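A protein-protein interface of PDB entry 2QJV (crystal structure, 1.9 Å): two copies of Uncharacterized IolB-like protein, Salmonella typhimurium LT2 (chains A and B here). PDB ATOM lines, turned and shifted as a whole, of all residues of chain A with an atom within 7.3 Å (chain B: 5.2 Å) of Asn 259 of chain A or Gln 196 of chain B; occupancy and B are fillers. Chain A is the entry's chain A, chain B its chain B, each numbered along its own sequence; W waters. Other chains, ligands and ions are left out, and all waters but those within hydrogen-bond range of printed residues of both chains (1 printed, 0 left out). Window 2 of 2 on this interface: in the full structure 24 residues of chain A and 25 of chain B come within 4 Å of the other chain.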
ATOM      1  N   TRP A 168       5.045  13.656   0.961  1.00  0.00           N
ATOM      2  CA  TRP A 168       3.816  13.840   0.246  1.00  0.00           C
ATOM      3  C   TRP A 168       3.962  13.185  -1.116  1.00  0.00           C
ATOM      4  O   TRP A 168       4.989  13.342  -1.745  1.00  0.00           O
ATOM      5  CB  TRP A 168       3.535  15.360   0.125  1.00  0.00           C
ATOM      6  CG  TRP A 168       2.330  15.701  -0.671  1.00  0.00           C
ATOM      7  CD1 TRP A 168       2.304  16.141  -1.961  1.00  0.00           C
ATOM      8  CD2 TRP A 168       0.964  15.626  -0.237  1.00  0.00           C
ATOM      9  NE1 TRP A 168       1.006  16.348  -2.362  1.00  0.00           N
ATOM     10  CE2 TRP A 168       0.160  16.048  -1.328  1.00  0.00           C
ATOM     11  CE3 TRP A 168       0.341  15.268   0.970  1.00  0.00           C
ATOM     12  CZ2 TRP A 168      -1.243  16.088  -1.258  1.00  0.00           C
ATOM     13  CZ3 TRP A 168      -1.038  15.302   1.043  1.00  0.00           C
ATOM     14  CH2 TRP A 168      -1.828  15.717  -0.061  1.00  0.00           C
ATOM     15  N   ASP A 206      -6.339   9.224   9.554  1.00  0.00           N
ATOM     16  CA  ASP A 206      -7.540   9.124   8.745  1.00  0.00           C
ATOM     17  C   ASP A 206      -8.827   9.573   9.469  1.00  0.00           C
ATOM     18  O   ASP A 206      -9.646  10.233   8.875  1.00  0.00           O
ATOM     19  CB  ASP A 206      -7.745   7.675   8.247  1.00  0.00           C
ATOM     20  CG  ASP A 206      -6.815   7.309   7.106  1.00  0.00           C
ATOM     21  OD1 ASP A 206      -6.995   7.881   5.990  1.00  0.00           O
ATOM     22  OD2 ASP A 206      -5.942   6.419   7.338  1.00  0.00           O
ATOM     23  N   ARG A 208      -8.919  11.707  11.927  1.00  0.00           N
ATOM     24  CA  ARG A 208      -8.643  13.049  12.458  1.00  0.00           C
ATOM     25  C   ARG A 208      -8.647  13.107  13.999  1.00  0.00           C
ATOM     26  O   ARG A 208      -8.725  14.201  14.572  1.00  0.00           O
ATOM     27  CB  ARG A 208      -9.626  14.094  11.899  1.00  0.00           C
ATOM     28  CG  ARG A 208      -9.907  13.994  10.406  1.00  0.00           C
ATOM     29  CD  ARG A 208      -8.658  14.100   9.572  1.00  0.00           C
ATOM     30  NE  ARG A 208      -8.935  13.860   8.154  1.00  0.00           N
ATOM     31  CZ  ARG A 208      -9.400  14.769   7.298  1.00  0.00           C
ATOM     32  NH1 ARG A 208      -9.685  16.017   7.695  1.00  0.00           N
ATOM     33  NH2 ARG A 208      -9.615  14.409   6.038  1.00  0.00           N
ATOM     34  N   TRP A 256      -0.093   4.748   1.706  1.00  0.00           N
ATOM     35  CA  TRP A 256      -0.524   6.053   1.231  1.00  0.00           C
ATOM     36  C   TRP A 256      -1.971   6.379   1.613  1.00  0.00           C
ATOM     37  O   TRP A 256      -2.813   5.512   1.583  1.00  0.00           O
ATOM     38  CB  TRP A 256      -0.404   6.146  -0.292  1.00  0.00           C
ATOM     39  CG  TRP A 256       0.981   6.517  -0.740  1.00  0.00           C
ATOM     40  CD1 TRP A 256       1.705   7.633  -0.381  1.00  0.00           C
ATOM     41  CD2 TRP A 256       1.762   5.823  -1.679  1.00  0.00           C
ATOM     42  NE1 TRP A 256       2.908   7.652  -1.020  1.00  0.00           N
ATOM     43  CE2 TRP A 256       2.970   6.551  -1.835  1.00  0.00           C
ATOM     44  CE3 TRP A 256       1.569   4.644  -2.407  1.00  0.00           C
ATOM     45  CZ2 TRP A 256       3.981   6.132  -2.679  1.00  0.00           C
ATOM     46  CZ3 TRP A 256       2.574   4.225  -3.252  1.00  0.00           C
ATOM     47  CH2 TRP A 256       3.775   4.969  -3.379  1.00  0.00           C
ATOM     48  N   GLU A 257      -2.240   7.629   2.003  1.00  0.00           N
ATOM     49  CA  GLU A 257      -3.615   8.094   2.232  1.00  0.00           C
ATOM     50  C   GLU A 257      -4.337   7.960   0.909  1.00  0.00           C
ATOM     51  O   GLU A 257      -3.861   8.446  -0.135  1.00  0.00           O
ATOM     52  CB  GLU A 257      -3.629   9.544   2.729  1.00  0.00           C
ATOM     53  CG  GLU A 257      -5.021  10.020   3.060  1.00  0.00           C
ATOM     54  CD  GLU A 257      -5.063  11.456   3.576  1.00  0.00           C
ATOM     55  OE1 GLU A 257      -4.019  12.129   3.573  1.00  0.00           O
ATOM     56  OE2 GLU A 257      -6.170  11.903   3.943  1.00  0.00           O
ATOM     57  N   GLU A 258      -5.476   7.277   0.914  1.00  0.00           N
ATOM     58  CA  GLU A 258      -6.134   6.916  -0.343  1.00  0.00           C
ATOM     59  C   GLU A 258      -6.539   8.113  -1.227  1.00  0.00           C
ATOM     60  O   GLU A 258      -6.418   8.049  -2.462  1.00  0.00           O
ATOM     61  CB  GLU A 258      -7.347   5.989  -0.098  1.00  0.00           C
ATOM     62  N   ASN A 259      -7.001   9.200  -0.606  1.00  0.00           N
ATOM     63  CA  ASN A 259      -7.465  10.370  -1.392  1.00  0.00           C
ATOM     64  C   ASN A 259      -6.423  11.085  -2.219  1.00  0.00           C
ATOM     65  O   ASN A 259      -6.767  11.737  -3.189  1.00  0.00           O
ATOM     66  CB  ASN A 259      -8.134  11.427  -0.478  1.00  0.00           C
ATOM     67  CG  ASN A 259      -9.644  11.217  -0.372  1.00  0.00           C
ATOM     68  OD1 ASN A 259     -10.169  11.042   0.712  1.00  0.00           O
ATOM     69  ND2 ASN A 259     -10.338  11.205  -1.522  1.00  0.00           N
ATOM     70  N   HIS A 260      -5.167  11.008  -1.789  1.00  0.00           N
ATOM     71  CA  HIS A 260      -4.066  11.697  -2.468  1.00  0.00           C
ATOM     72  C   HIS A 260      -3.102  10.777  -3.231  1.00  0.00           C
ATOM     73  O   HIS A 260      -2.158  11.287  -3.849  1.00  0.00           O
ATOM     74  CB  HIS A 260      -3.311  12.531  -1.434  1.00  0.00           C
ATOM     75  CG  HIS A 260      -4.234  13.284  -0.531  1.00  0.00           C
ATOM     76  ND1 HIS A 260      -5.252  14.096  -1.008  1.00  0.00           N
ATOM     77  CD2 HIS A 260      -4.311  13.329   0.813  1.00  0.00           C
ATOM     78  CE1 HIS A 260      -5.917  14.599   0.017  1.00  0.00           C
ATOM     79  NE2 HIS A 260      -5.354  14.164   1.130  1.00  0.00           N
ATOM     80  N   ALA A 261      -3.373   9.458  -3.224  1.00  0.00           N
ATOM     81  CA  ALA A 261      -2.488   8.459  -3.845  1.00  0.00           C
ATOM     82  C   ALA A 261      -2.302   8.720  -5.352  1.00  0.00           C
ATOM     83  O   ALA A 261      -1.231   8.420  -5.876  1.00  0.00           O
ATOM     84  CB  ALA A 261      -3.000   7.019  -3.565  1.00  0.00           C
ATOM     85  N   TRP A 262      -3.319   9.301  -6.019  1.00  0.00           N
ATOM     86  CA  TRP A 262      -3.255   9.671  -7.450  1.00  0.00           C
ATOM     87  C   TRP A 262      -2.077  10.588  -7.842  1.00  0.00           C
ATOM     88  O   TRP A 262      -1.703  10.630  -9.013  1.00  0.00           O
ATOM     89  CB  TRP A 262      -4.576  10.338  -7.931  1.00  0.00           C
ATOM     90  CG  TRP A 262      -4.799  11.709  -7.323  1.00  0.00           C
ATOM     91  CD1 TRP A 262      -5.388  11.982  -6.112  1.00  0.00           C
ATOM     92  CD2 TRP A 262      -4.393  12.978  -7.872  1.00  0.00           C
ATOM     93  NE1 TRP A 262      -5.372  13.337  -5.880  1.00  0.00           N
ATOM     94  CE2 TRP A 262      -4.776  13.978  -6.937  1.00  0.00           C
ATOM     95  CE3 TRP A 262      -3.748  13.371  -9.061  1.00  0.00           C
ATOM     96  CZ2 TRP A 262      -4.524  15.344  -7.151  1.00  0.00           C
ATOM     97  CZ3 TRP A 262      -3.499  14.739  -9.280  1.00  0.00           C
ATOM     98  CH2 TRP A 262      -3.897  15.711  -8.335  1.00  0.00           C
ATOM     99  N   ILE A 263      -1.544  11.349  -6.889  1.00  0.00           N
ATOM    100  CA  ILE A 263      -0.419  12.268  -7.118  1.00  0.00           C
ATOM    101  C   ILE A 263       0.882  11.471  -7.475  1.00  0.00           C
ATOM    102  O   ILE A 263       1.782  12.019  -8.119  1.00  0.00           O
ATOM    103  CB  ILE A 263      -0.257  13.272  -5.907  1.00  0.00           C
ATOM    104  CG1 ILE A 263      -1.523  14.154  -5.750  1.00  0.00           C
ATOM    105  CG2 ILE A 263       0.994  14.157  -6.042  1.00  0.00           C
ATOM    106  CD1 ILE A 263      -1.559  15.024  -4.493  1.00  0.00           C
ATOM    107  N   PRO B 194      -8.226  19.342  -7.577  1.00  0.00           N
ATOM    108  CA  PRO B 194      -9.446  18.545  -7.355  1.00  0.00           C
ATOM    109  C   PRO B 194     -10.065  18.823  -5.978  1.00  0.00           C
ATOM    110  O   PRO B 194      -9.366  19.327  -5.044  1.00  0.00           O
ATOM    111  CB  PRO B 194      -8.976  17.083  -7.517  1.00  0.00           C
ATOM    112  CG  PRO B 194      -7.725  17.169  -8.284  1.00  0.00           C
ATOM    113  CD  PRO B 194      -7.072  18.481  -7.869  1.00  0.00           C
ATOM    114  N   PRO B 195     -11.368  18.523  -5.840  1.00  0.00           N
ATOM    115  CA  PRO B 195     -12.152  18.919  -4.653  1.00  0.00           C
ATOM    116  C   PRO B 195     -11.775  18.314  -3.287  1.00  0.00           C
ATOM    117  O   PRO B 195     -12.074  18.927  -2.252  1.00  0.00           O
ATOM    118  CB  PRO B 195     -13.615  18.526  -5.055  1.00  0.00           C
ATOM    119  CG  PRO B 195     -13.508  17.616  -6.150  1.00  0.00           C
ATOM    120  CD  PRO B 195     -12.200  17.826  -6.842  1.00  0.00           C
ATOM    121  N   GLN B 196     -11.084  17.177  -3.276  1.00  0.00           N
ATOM    122  CA  GLN B 196     -10.697  16.493  -2.015  1.00  0.00           C
ATOM    123  C   GLN B 196      -9.418  17.102  -1.358  1.00  0.00           C
ATOM    124  O   GLN B 196      -8.953  16.599  -0.333  1.00  0.00           O
ATOM    125  CB  GLN B 196     -10.555  14.946  -2.201  1.00  0.00           C
ATOM    126  CG  GLN B 196      -9.312  14.411  -2.946  1.00  0.00           C
ATOM    127  CD  GLN B 196      -9.423  14.388  -4.452  1.00  0.00           C
ATOM    128  OE1 GLN B 196     -10.182  15.158  -5.062  1.00  0.00           O
ATOM    129  NE2 GLN B 196      -8.641  13.506  -5.074  1.00  0.00           N
ATOM    130  N   GLY B 197      -8.863  18.166  -1.955  1.00  0.00           N
ATOM    131  CA  GLY B 197      -7.647  18.790  -1.440  1.00  0.00           C
ATOM    132  C   GLY B 197      -7.777  19.609  -0.181  1.00  0.00           C
ATOM    133  O   GLY B 197      -8.862  19.818   0.338  1.00  0.00           O
ATOM    134  N   PHE B 198      -6.628  20.089   0.285  1.00  0.00           N
ATOM    135  CA  PHE B 198      -6.561  20.965   1.422  1.00  0.00           C
ATOM    136  C   PHE B 198      -5.338  21.881   1.251  1.00  0.00           C
ATOM    137  O   PHE B 198      -4.506  21.673   0.349  1.00  0.00           O
ATOM    138  CB  PHE B 198      -6.545  20.180   2.772  1.00  0.00           C
ATOM    139  CG  PHE B 198      -5.290  19.408   3.017  1.00  0.00           C
ATOM    140  CD1 PHE B 198      -4.208  19.999   3.666  1.00  0.00           C
ATOM    141  CD2 PHE B 198      -5.178  18.089   2.604  1.00  0.00           C
ATOM    142  CE1 PHE B 198      -3.041  19.289   3.875  1.00  0.00           C
ATOM    143  CE2 PHE B 198      -4.017  17.367   2.834  1.00  0.00           C
ATOM    144  CZ  PHE B 198      -2.936  17.988   3.457  1.00  0.00           C
ATOM    145  N   TYR B 217     -10.177  22.442   4.112  1.00  0.00           N
ATOM    146  CA  TYR B 217     -10.709  21.634   3.034  1.00  0.00           C
ATOM    147  C   TYR B 217     -11.790  22.400   2.249  1.00  0.00           C
ATOM    148  O   TYR B 217     -12.092  23.534   2.551  1.00  0.00           O
ATOM    149  CB  TYR B 217     -11.225  20.298   3.593  1.00  0.00           C
ATOM    150  CG  TYR B 217     -10.144  19.312   4.022  1.00  0.00           C
ATOM    151  CD1 TYR B 217      -9.408  19.484   5.230  1.00  0.00           C
ATOM    152  CD2 TYR B 217      -9.880  18.177   3.253  1.00  0.00           C
ATOM    153  CE1 TYR B 217      -8.414  18.559   5.601  1.00  0.00           C
ATOM    154  CE2 TYR B 217      -8.911  17.261   3.621  1.00  0.00           C
ATOM    155  CZ  TYR B 217      -8.174  17.443   4.780  1.00  0.00           C
ATOM    156  OH  TYR B 217      -7.242  16.455   5.064  1.00  0.00           O
ATOM    157  N   TYR B 237      -3.076  20.218  -5.541  1.00  0.00           N
ATOM    158  CA  TYR B 237      -4.348  20.862  -5.221  1.00  0.00           C
ATOM    159  C   TYR B 237      -4.336  22.381  -5.383  1.00  0.00           C
ATOM    160  O   TYR B 237      -3.851  23.116  -4.516  1.00  0.00           O
ATOM    161  CB  TYR B 237      -4.775  20.493  -3.797  1.00  0.00           C
ATOM    162  CG  TYR B 237      -5.067  19.022  -3.666  1.00  0.00           C
ATOM    163  CD1 TYR B 237      -6.150  18.465  -4.349  1.00  0.00           C
ATOM    164  CD2 TYR B 237      -4.289  18.187  -2.878  1.00  0.00           C
ATOM    165  CE1 TYR B 237      -6.449  17.115  -4.249  1.00  0.00           C
ATOM    166  CE2 TYR B 237      -4.583  16.827  -2.787  1.00  0.00           C
ATOM    167  CZ  TYR B 237      -5.663  16.309  -3.472  1.00  0.00           C
ATOM    168  OH  TYR B 237      -5.982  14.984  -3.405  1.00  0.00           O
HETATM  169  O   HOH W   1      -6.844  14.400   3.493  1.00  0.00           O
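The guanidinium group of Arg 208 of chain A is in hydrogen-bond range of the side-chain hydroxyl of Tyr 217 of chain B (3.3 Å).
The side-chain amide nitrogen (NE2) of Gln 196 of chain B sits at hydrogen-bond distance from the backbone carbonyl oxygen (O) of Asn 259 of chain A, at 3.2 Å.
The side-chain hydroxyl (OH) of Tyr 237 of chain B is in hydrogen-bond range of the backbone carbonyl oxygen (O) of Asn 259 of chain A, at 3.3 Å.
A ring nitrogen (ND1) of His 260 of chain A sits at hydrogen-bond distance from the side-chain hydroxyl of Tyr 237 of chain B, 2.7 Å away.
The indole nitrogen (NE1) of Trp 262 of chain A lies close to the side-chain amide nitrogen (NE2) of Gln 196 of chain B (3.4 Å).
The indole nitrogen (NE1) of Trp 262 of chain A sits at hydrogen-bond distance from the side-chain hydroxyl (OH) of Tyr 237 of chain B (3.0 Å).
No position is printed for both chains.
Of the 12 pairs that touch across the chains among the printed residues, none has its exchanged pair printed and touching as well.
CH2 of Trp 168 of chain A touches CE2 of Phe 198 of chain B, at 3.99 Å.
Trp 168 of chain A touches Tyr 237 of chain B.
O of Gln 196 of chain B touches CE1 of His 260 of chain A, at 3.7 Å.
Phe 198 of chain B touches His 260 of chain A (CE2 to NE2, 3.9 Å).
CZ2 of Trp 262 of chain A touches CG of Pro 194 of chain B, at 3.9 Å.
Tyr 237 of chain B touches Ile 263 of chain A (CE2 to CD1, 3.9 Å).
Asn 259 of chain A touches two residues of chain B.
Gln 196 of chain B touches three residues of chain A.
Of the printed residues of chain B, Arg 208 of chain A touches Tyr 217 (3.3 Å).
Printed residues of chain A within 4 Å of Phe 198 of chain B: Trp 168 (3.99 Å) and His 260 (3.9 Å).
Of the printed residues of chain B, His 260 of chain A touches Gln 196 (3.7 Å), Phe 198 (3.9 Å) and Tyr 237 (2.7 Å).
Glu 257 of chain A touches none of the printed residues of chain B.
Pro 195 of chain B touches none of the printed residues of chain A.
The nearest printed residue of chain B that does not touch Asn 259 of chain A is Gly 197 of chain B (6.9 Å).
The nearest residue of chain A that does not touch Gln 196 of chain B is Glu 258 of chain A (6.4 Å).
The nearest printed residue of chain B that does not touch Trp 168 of chain A is Gly 197 of chain B (6.7 Å).
The side-chain carboxylate of Glu 257 of chain A sits close to a ring nitrogen (NE2) of His 260 of chain A, at 3.4 Å.
O of Asn 259 of chain A lies close to NE1 of Trp 262 of chain A, 3.4 Å away.
The side-chain hydroxyl (OH) of Tyr 237 of chain B sits close to the side-chain amide nitrogen (NE2) of Gln 196 of chain B, at 3.5 Å.
Water W1 lies within hydrogen-bond range of the side-chain hydroxyl of Tyr 217 of chain B (2.6 Å), the side-chain carboxylate of Glu 257 of chain A (2.6 Å) and a ring nitrogen (NE2) of His 260 of chain A (2.8 Å).
Of the 11 printed residues of chain A, 6 touch a printed residue of chain B.
Printed residues of chain A that touch a printed residue of chain B: Trp 168, Arg 208, Asn 259, His 260, Trp 262 and Ile 263.
Hydrophobic or aromatic side chains of chain A within 4 Å of the printed part of chain B: Trp 168, His 260, Trp 262 and Ile 263.
Of the 7 printed residues of chain B, 5 touch a printed residue of chain A.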
